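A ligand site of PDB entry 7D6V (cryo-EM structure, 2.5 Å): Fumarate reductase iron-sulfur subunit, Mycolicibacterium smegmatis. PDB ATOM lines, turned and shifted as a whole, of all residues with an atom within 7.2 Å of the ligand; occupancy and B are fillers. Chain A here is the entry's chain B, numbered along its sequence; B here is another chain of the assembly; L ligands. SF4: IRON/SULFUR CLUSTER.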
ATOM      1  N   GLY A  60      10.091 -27.924  15.311  1.00  0.00           N
ATOM      2  CA  GLY A  60      11.132 -28.841  15.736  1.00  0.00           C
ATOM      3  C   GLY A  60      10.905 -30.334  15.664  1.00  0.00           C
ATOM      4  O   GLY A  60      11.725 -31.105  16.154  1.00  0.00           O
ATOM      5  N   SER A  63      13.340 -32.649  12.630  1.00  0.00           N
ATOM      6  CA  SER A  63      14.790 -32.552  12.583  1.00  0.00           C
ATOM      7  C   SER A  63      15.397 -33.821  12.012  1.00  0.00           C
ATOM      8  O   SER A  63      15.067 -34.938  12.444  1.00  0.00           O
ATOM      9  CB  SER A  63      15.340 -32.290  13.984  1.00  0.00           C
ATOM     10  OG  SER A  63      14.794 -31.103  14.527  1.00  0.00           O
ATOM     11  N   LEU A  72      15.887 -29.002   9.199  1.00  0.00           N
ATOM     12  CA  LEU A  72      14.479 -29.341   9.287  1.00  0.00           C
ATOM     13  C   LEU A  72      14.011 -29.805   7.916  1.00  0.00           C
ATOM     14  O   LEU A  72      14.298 -29.163   6.905  1.00  0.00           O
ATOM     15  CB  LEU A  72      13.642 -28.139   9.744  1.00  0.00           C
ATOM     16  CG  LEU A  72      13.842 -27.577  11.145  1.00  0.00           C
ATOM     17  CD1 LEU A  72      13.053 -26.297  11.302  1.00  0.00           C
ATOM     18  CD2 LEU A  72      13.432 -28.592  12.200  1.00  0.00           C
ATOM     19  N   PHE A 142      16.181 -15.199  22.942  1.00  0.00           N
ATOM     20  CA  PHE A 142      16.306 -16.614  23.242  1.00  0.00           C
ATOM     21  C   PHE A 142      14.959 -17.306  23.347  1.00  0.00           C
ATOM     22  O   PHE A 142      14.891 -18.530  23.206  1.00  0.00           O
ATOM     23  CB  PHE A 142      17.085 -16.821  24.539  1.00  0.00           C
ATOM     24  CG  PHE A 142      18.378 -16.068  24.594  1.00  0.00           C
ATOM     25  CD1 PHE A 142      19.204 -15.995  23.487  1.00  0.00           C
ATOM     26  CD2 PHE A 142      18.777 -15.436  25.759  1.00  0.00           C
ATOM     27  CE1 PHE A 142      20.390 -15.299  23.534  1.00  0.00           C
ATOM     28  CE2 PHE A 142      19.964 -14.743  25.815  1.00  0.00           C
ATOM     29  CZ  PHE A 142      20.772 -14.677  24.708  1.00  0.00           C
ATOM     30  N   LYS A 144      12.783 -17.244  21.196  1.00  0.00           N
ATOM     31  CA  LYS A 144      12.398 -17.644  19.849  1.00  0.00           C
ATOM     32  C   LYS A 144      12.639 -19.112  19.573  1.00  0.00           C
ATOM     33  O   LYS A 144      12.243 -19.602  18.507  1.00  0.00           O
ATOM     34  CB  LYS A 144      13.172 -16.818  18.813  1.00  0.00           C
ATOM     35  CG  LYS A 144      12.630 -15.426  18.570  1.00  0.00           C
ATOM     36  CD  LYS A 144      13.697 -14.534  17.964  1.00  0.00           C
ATOM     37  CE  LYS A 144      14.247 -15.151  16.691  1.00  0.00           C
ATOM     38  NZ  LYS A 144      15.694 -14.834  16.503  1.00  0.00           N
ATOM     39  N   CYS A 145      13.311 -19.797  20.483  1.00  0.00           N
ATOM     40  CA  CYS A 145      13.716 -21.188  20.269  1.00  0.00           C
ATOM     41  C   CYS A 145      12.684 -22.321  20.140  1.00  0.00           C
ATOM     42  O   CYS A 145      12.144 -22.787  21.144  1.00  0.00           O
ATOM     43  CB  CYS A 145      14.766 -21.591  21.314  1.00  0.00           C
ATOM     44  SG  CYS A 145      14.835 -23.359  21.668  1.00  0.00           S
ATOM     45  N   ILE A 146      12.432 -22.769  18.909  1.00  0.00           N
ATOM     46  CA  ILE A 146      11.583 -23.938  18.720  1.00  0.00           C
ATOM     47  C   ILE A 146      12.440 -25.146  19.057  1.00  0.00           C
ATOM     48  O   ILE A 146      13.525 -25.332  18.496  1.00  0.00           O
ATOM     49  CB  ILE A 146      11.020 -24.012  17.297  1.00  0.00           C
ATOM     50  CG1 ILE A 146      12.114 -24.188  16.241  1.00  0.00           C
ATOM     51  CG2 ILE A 146      10.227 -22.747  16.984  1.00  0.00           C
ATOM     52  CD1 ILE A 146      11.622 -24.736  14.938  1.00  0.00           C
ATOM     53  N   GLU A 147      11.991 -25.959  20.012  1.00  0.00           N
ATOM     54  CA  GLU A 147      12.895 -26.968  20.539  1.00  0.00           C
ATOM     55  C   GLU A 147      13.119 -28.078  19.529  1.00  0.00           C
ATOM     56  O   GLU A 147      12.595 -29.182  19.668  1.00  0.00           O
ATOM     57  CB  GLU A 147      12.367 -27.500  21.862  1.00  0.00           C
ATOM     58  CG  GLU A 147      12.566 -26.540  23.007  1.00  0.00           C
ATOM     59  CD  GLU A 147      12.009 -27.049  24.309  1.00  0.00           C
ATOM     60  OE1 GLU A 147      11.052 -27.854  24.276  1.00  0.00           O
ATOM     61  OE2 GLU A 147      12.521 -26.646  25.381  1.00  0.00           O
ATOM     62  N   CYS A 148      13.922 -27.787  18.508  1.00  0.00           N
ATOM     63  CA  CYS A 148      14.236 -28.763  17.473  1.00  0.00           C
ATOM     64  C   CYS A 148      15.402 -29.642  17.940  1.00  0.00           C
ATOM     65  O   CYS A 148      15.477 -30.818  17.594  1.00  0.00           O
ATOM     66  CB  CYS A 148      14.590 -28.068  16.161  1.00  0.00           C
ATOM     67  SG  CYS A 148      16.335 -27.602  16.003  1.00  0.00           S
ATOM     68  N   PHE A 149      16.304 -29.050  18.709  1.00  0.00           N
ATOM     69  CA  PHE A 149      17.476 -29.766  19.227  1.00  0.00           C
ATOM     70  C   PHE A 149      18.512 -30.049  18.159  1.00  0.00           C
ATOM     71  O   PHE A 149      19.330 -30.961  18.314  1.00  0.00           O
ATOM     72  CB  PHE A 149      17.049 -31.062  19.938  1.00  0.00           C
ATOM     73  CG  PHE A 149      15.988 -30.857  20.979  1.00  0.00           C
ATOM     74  CD1 PHE A 149      16.127 -29.875  21.946  1.00  0.00           C
ATOM     75  CD2 PHE A 149      14.848 -31.624  20.974  1.00  0.00           C
ATOM     76  CE1 PHE A 149      15.155 -29.684  22.905  1.00  0.00           C
ATOM     77  CE2 PHE A 149      13.869 -31.444  21.929  1.00  0.00           C
ATOM     78  CZ  PHE A 149      14.021 -30.468  22.892  1.00  0.00           C
ATOM     79  N   LEU A 150      18.505 -29.293  17.070  1.00  0.00           N
ATOM     80  CA  LEU A 150      19.552 -29.428  16.069  1.00  0.00           C
ATOM     81  C   LEU A 150      20.892 -28.962  16.612  1.00  0.00           C
ATOM     82  O   LEU A 150      21.943 -29.536  16.283  1.00  0.00           O
ATOM     83  CB  LEU A 150      19.177 -28.648  14.811  1.00  0.00           C
ATOM     84  CG  LEU A 150      18.073 -29.239  13.928  1.00  0.00           C
ATOM     85  CD1 LEU A 150      17.669 -28.260  12.848  1.00  0.00           C
ATOM     86  CD2 LEU A 150      18.498 -30.563  13.338  1.00  0.00           C
ATOM     87  N   CYS A 151      20.848 -27.971  17.488  1.00  0.00           N
ATOM     88  CA  CYS A 151      22.054 -27.458  18.132  1.00  0.00           C
ATOM     89  C   CYS A 151      22.625 -28.581  18.993  1.00  0.00           C
ATOM     90  O   CYS A 151      23.823 -28.852  18.956  1.00  0.00           O
ATOM     91  CB  CYS A 151      21.736 -26.232  18.983  1.00  0.00           C
ATOM     92  SG  CYS A 151      20.604 -26.553  20.359  1.00  0.00           S
ATOM     93  N   GLN A 152      21.755 -29.218  19.780  1.00  0.00           N
ATOM     94  CA  GLN A 152      22.174 -30.330  20.623  1.00  0.00           C
ATOM     95  C   GLN A 152      22.735 -31.464  19.786  1.00  0.00           C
ATOM     96  O   GLN A 152      23.687 -32.129  20.191  1.00  0.00           O
ATOM     97  CB  GLN A 152      20.994 -30.810  21.458  1.00  0.00           C
ATOM     98  CG  GLN A 152      20.258 -29.721  22.204  1.00  0.00           C
ATOM     99  CD  GLN A 152      20.875 -29.439  23.561  1.00  0.00           C
ATOM    100  OE1 GLN A 152      21.405 -28.355  23.791  1.00  0.00           O
ATOM    101  NE2 GLN A 152      20.811 -30.411  24.457  1.00  0.00           N
ATOM    102  N   PRO A 171      23.977 -26.656  24.000  1.00  0.00           N
ATOM    103  CA  PRO A 171      23.727 -25.249  23.671  1.00  0.00           C
ATOM    104  C   PRO A 171      22.353 -24.750  24.045  1.00  0.00           C
ATOM    105  O   PRO A 171      22.228 -23.615  24.523  1.00  0.00           O
ATOM    106  CB  PRO A 171      23.935 -25.222  22.141  1.00  0.00           C
ATOM    107  CG  PRO A 171      24.066 -26.646  21.702  1.00  0.00           C
ATOM    108  CD  PRO A 171      24.534 -27.415  22.876  1.00  0.00           C
ATOM    109  N   ARG A 172      21.309 -25.547  23.843  1.00  0.00           N
ATOM    110  CA  ARG A 172      19.946 -25.079  24.086  1.00  0.00           C
ATOM    111  C   ARG A 172      19.737 -24.712  25.552  1.00  0.00           C
ATOM    112  O   ARG A 172      19.151 -23.680  25.867  1.00  0.00           O
ATOM    113  CB  ARG A 172      18.927 -26.128  23.642  1.00  0.00           C
ATOM    114  CG  ARG A 172      17.489 -25.653  23.595  1.00  0.00           C
ATOM    115  CD  ARG A 172      16.735 -26.025  24.869  1.00  0.00           C
ATOM    116  NE  ARG A 172      15.423 -25.400  24.949  1.00  0.00           N
ATOM    117  CZ  ARG A 172      15.208 -24.128  25.276  1.00  0.00           C
ATOM    118  NH1 ARG A 172      13.972 -23.656  25.320  1.00  0.00           N
ATOM    119  NH2 ARG A 172      16.221 -23.332  25.558  1.00  0.00           N
ATOM    120  N   MET A 175      21.766 -21.749  26.711  1.00  0.00           N
ATOM    121  CA  MET A 175      21.003 -20.600  26.242  1.00  0.00           C
ATOM    122  C   MET A 175      19.811 -20.323  27.144  1.00  0.00           C
ATOM    123  O   MET A 175      19.468 -19.169  27.399  1.00  0.00           O
ATOM    124  CB  MET A 175      20.553 -20.811  24.804  1.00  0.00           C
ATOM    125  CG  MET A 175      19.844 -19.632  24.177  1.00  0.00           C
ATOM    126  SD  MET A 175      19.084 -20.019  22.604  1.00  0.00           S
ATOM    127  CE  MET A 175      17.810 -21.163  23.119  1.00  0.00           C
ATOM    128  N   CYS A 209      27.010 -24.745  16.440  1.00  0.00           N
ATOM    129  CA  CYS A 209      25.597 -24.708  16.815  1.00  0.00           C
ATOM    130  C   CYS A 209      24.875 -23.552  16.072  1.00  0.00           C
ATOM    131  O   CYS A 209      24.014 -23.808  15.222  1.00  0.00           O
ATOM    132  CB  CYS A 209      25.443 -24.526  18.331  1.00  0.00           C
ATOM    133  SG  CYS A 209      25.953 -22.909  18.955  1.00  0.00           S
ATOM    134  N   THR A 210      25.221 -22.307  16.389  1.00  0.00           N
ATOM    135  CA  THR A 210      24.700 -21.180  15.825  1.00  0.00           C
ATOM    136  C   THR A 210      24.645 -21.432  14.459  1.00  0.00           C
ATOM    137  O   THR A 210      23.857 -20.874  13.851  1.00  0.00           O
ATOM    138  CB  THR A 210      25.756 -20.113  15.860  1.00  0.00           C
ATOM    139  OG1 THR A 210      25.871 -19.701  17.117  1.00  0.00           O
ATOM    140  CG2 THR A 210      25.382 -18.924  15.246  1.00  0.00           C
ATOM    141  N   VAL A 212      23.540 -24.032  12.843  1.00  0.00           N
ATOM    142  CA  VAL A 212      22.457 -24.928  12.445  1.00  0.00           C
ATOM    143  C   VAL A 212      21.093 -24.431  12.883  1.00  0.00           C
ATOM    144  O   VAL A 212      20.082 -25.047  12.530  1.00  0.00           O
ATOM    145  CB  VAL A 212      22.691 -26.354  12.964  1.00  0.00           C
ATOM    146  CG1 VAL A 212      23.992 -26.914  12.434  1.00  0.00           C
ATOM    147  CG2 VAL A 212      22.670 -26.369  14.485  1.00  0.00           C
ATOM    148  N   CYS A 213      21.048 -23.375  13.687  1.00  0.00           N
ATOM    149  CA  CYS A 213      19.770 -22.880  14.199  1.00  0.00           C
ATOM    150  C   CYS A 213      18.796 -22.361  13.135  1.00  0.00           C
ATOM    151  O   CYS A 213      19.079 -21.380  12.451  1.00  0.00           O
ATOM    152  CB  CYS A 213      20.015 -21.779  15.241  1.00  0.00           C
ATOM    153  SG  CYS A 213      18.523 -20.884  15.742  1.00  0.00           S
ATOM    154  N   PRO A 214      17.646 -23.037  12.993  1.00  0.00           N
ATOM    155  CA  PRO A 214      16.670 -22.542  12.007  1.00  0.00           C
ATOM    156  C   PRO A 214      16.097 -21.187  12.380  1.00  0.00           C
ATOM    157  O   PRO A 214      15.590 -20.490  11.496  1.00  0.00           O
ATOM    158  CB  PRO A 214      15.585 -23.617  11.993  1.00  0.00           C
ATOM    159  CG  PRO A 214      16.148 -24.774  12.768  1.00  0.00           C
ATOM    160  CD  PRO A 214      17.132 -24.206  13.711  1.00  0.00           C
ATOM    161  N   GLU A 215      16.151 -20.810  13.643  1.00  0.00           N
ATOM    162  CA  GLU A 215      15.627 -19.536  14.108  1.00  0.00           C
ATOM    163  C   GLU A 215      16.656 -18.422  14.068  1.00  0.00           C
ATOM    164  O   GLU A 215      16.328 -17.280  14.391  1.00  0.00           O
ATOM    165  CB  GLU A 215      15.080 -19.681  15.529  1.00  0.00           C
ATOM    166  CG  GLU A 215      13.923 -20.644  15.645  1.00  0.00           C
ATOM    167  CD  GLU A 215      12.825 -20.344  14.642  1.00  0.00           C
ATOM    168  OE1 GLU A 215      12.440 -21.262  13.884  1.00  0.00           O
ATOM    169  OE2 GLU A 215      12.346 -19.193  14.610  1.00  0.00           O
ATOM    170  N   HIS A 216      17.899 -18.726  13.667  1.00  0.00           N
ATOM    171  CA  HIS A 216      18.966 -17.750  13.525  1.00  0.00           C
ATOM    172  C   HIS A 216      19.236 -17.022  14.841  1.00  0.00           C
ATOM    173  O   HIS A 216      19.488 -15.810  14.866  1.00  0.00           O
ATOM    174  CB  HIS A 216      18.653 -16.756  12.407  1.00  0.00           C
ATOM    175  CG  HIS A 216      18.250 -17.408  11.127  1.00  0.00           C
ATOM    176  ND1 HIS A 216      19.099 -18.218  10.409  1.00  0.00           N
ATOM    177  CD2 HIS A 216      17.088 -17.382  10.437  1.00  0.00           C
ATOM    178  CE1 HIS A 216      18.473 -18.657   9.328  1.00  0.00           C
ATOM    179  NE2 HIS A 216      17.254 -18.173   9.331  1.00  0.00           N
ATOM    180  N   ILE A 217      19.187 -17.769  15.941  1.00  0.00           N
ATOM    181  CA  ILE A 217      19.577 -17.233  17.242  1.00  0.00           C
ATOM    182  C   ILE A 217      21.097 -17.215  17.329  1.00  0.00           C
ATOM    183  O   ILE A 217      21.760 -18.194  16.981  1.00  0.00           O
ATOM    184  CB  ILE A 217      18.955 -18.069  18.373  1.00  0.00           C
ATOM    185  CG1 ILE A 217      17.446 -18.206  18.174  1.00  0.00           C
ATOM    186  CG2 ILE A 217      19.272 -17.446  19.729  1.00  0.00           C
ATOM    187  CD1 ILE A 217      16.789 -19.154  19.137  1.00  0.00           C
ATOM    188  N   ILE A 219      23.495 -17.967  19.216  1.00  0.00           N
ATOM    189  CA  ILE A 219      23.653 -18.760  20.433  1.00  0.00           C
ATOM    190  C   ILE A 219      25.009 -18.494  21.081  1.00  0.00           C
ATOM    191  O   ILE A 219      25.102 -18.227  22.285  1.00  0.00           O
ATOM    192  CB  ILE A 219      23.455 -20.246  20.133  1.00  0.00           C
ATOM    193  CG1 ILE A 219      22.119 -20.478  19.421  1.00  0.00           C
ATOM    194  CG2 ILE A 219      23.536 -21.061  21.416  1.00  0.00           C
ATOM    195  CD1 ILE A 219      21.935 -21.880  18.913  1.00  0.00           C
ATOM    196  N   ARG B 142       5.394 -22.382  25.415  1.00  0.00           N
ATOM    197  CA  ARG B 142       6.654 -22.476  26.130  1.00  0.00           C
ATOM    198  C   ARG B 142       6.470 -22.148  27.600  1.00  0.00           C
ATOM    199  O   ARG B 142       6.989 -22.851  28.480  1.00  0.00           O
ATOM    200  CB  ARG B 142       7.694 -21.537  25.524  1.00  0.00           C
ATOM    201  CG  ARG B 142       8.505 -22.117  24.403  1.00  0.00           C
ATOM    202  CD  ARG B 142       9.412 -23.252  24.827  1.00  0.00           C
ATOM    203  NE  ARG B 142       9.901 -23.940  23.642  1.00  0.00           N
ATOM    204  CZ  ARG B 142       9.199 -24.831  22.958  1.00  0.00           C
ATOM    205  NH1 ARG B 142       7.991 -25.166  23.356  1.00  0.00           N
ATOM    206  NH2 ARG B 142       9.709 -25.395  21.873  1.00  0.00           N
HETATM  207 FE1  SF4 L   1      18.916 -25.207  19.213  1.00  0.00          FE
HETATM  208 FE2  SF4 L   1      17.946 -22.881  17.552  1.00  0.00          FE
HETATM  209 FE3  SF4 L   1      16.242 -23.936  19.811  1.00  0.00          FE
HETATM  210 FE4  SF4 L   1      16.613 -25.570  17.303  1.00  0.00          FE
HETATM  211  S1  SF4 L   1      15.939 -23.596  17.725  1.00  0.00           S
HETATM  212  S2  SF4 L   1      16.919 -25.919  19.386  1.00  0.00           S
HETATM  213  S3  SF4 L   1      18.610 -24.859  17.130  1.00  0.00           S
HETATM  214  S4  SF4 L   1      18.249 -23.221  19.638  1.00  0.00           S
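Residues that only touch the ligand: Pro 214 (3.8 Å) and Ile 219 (3.99 Å). Eight residues have an atom within 4 Å of the ligand: Cys 145, Ile 146, Cys 148, Phe 149, Cys 151, Cys 213, Pro 214 and Ile 219. The nearest printed residue that does not touch the ligand is Met 175 (4.1 Å).
The side-chain hydroxyl (OG) of Ser 63 is in hydrogen-bond range of the backbone carbonyl oxygen (O) of Cys 148 (3.2 Å). The side-chain sulfur (SG) of Cys 151 lies close to the backbone NH (N) of Arg 172 (3.7 Å). N of His 216 sits close to SG of Cys 213. SG of Cys 145 lies close to NH1 of Arg 172, 3.8 Å away. The backbone NH (N) of Ile 217 lies close to the side-chain sulfur (SG) of Cys 213, at 3.2 Å. The backbone NH (N) of Leu 150 lies close to the side-chain sulfur (SG) of Cys 148, at 3.0 Å. SG of Cys 213 sits close to N of Glu 215 (3.2 Å).
An iron atom (FE3) of the ligand is bound by the side-chain sulfur of Cys 145 (2.4 Å). The backbone NH (N) of Cys 148 lies close to a sulfur (S2) of the ligand, at 3.6 Å. SG of Cys 213 is bound to FE2 of the ligand (2.8 Å). FE1 of the ligand is bound by SG of Cys 151. The backbone NH (N) of Phe 149 sits close to a sulfur (S2) of the ligand, at 3.3 Å. FE4 of the ligand is bound by SG of Cys 148, 2.4 Å away. N of Ile 146 sits close to S1 of the ligand (3.8 Å).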
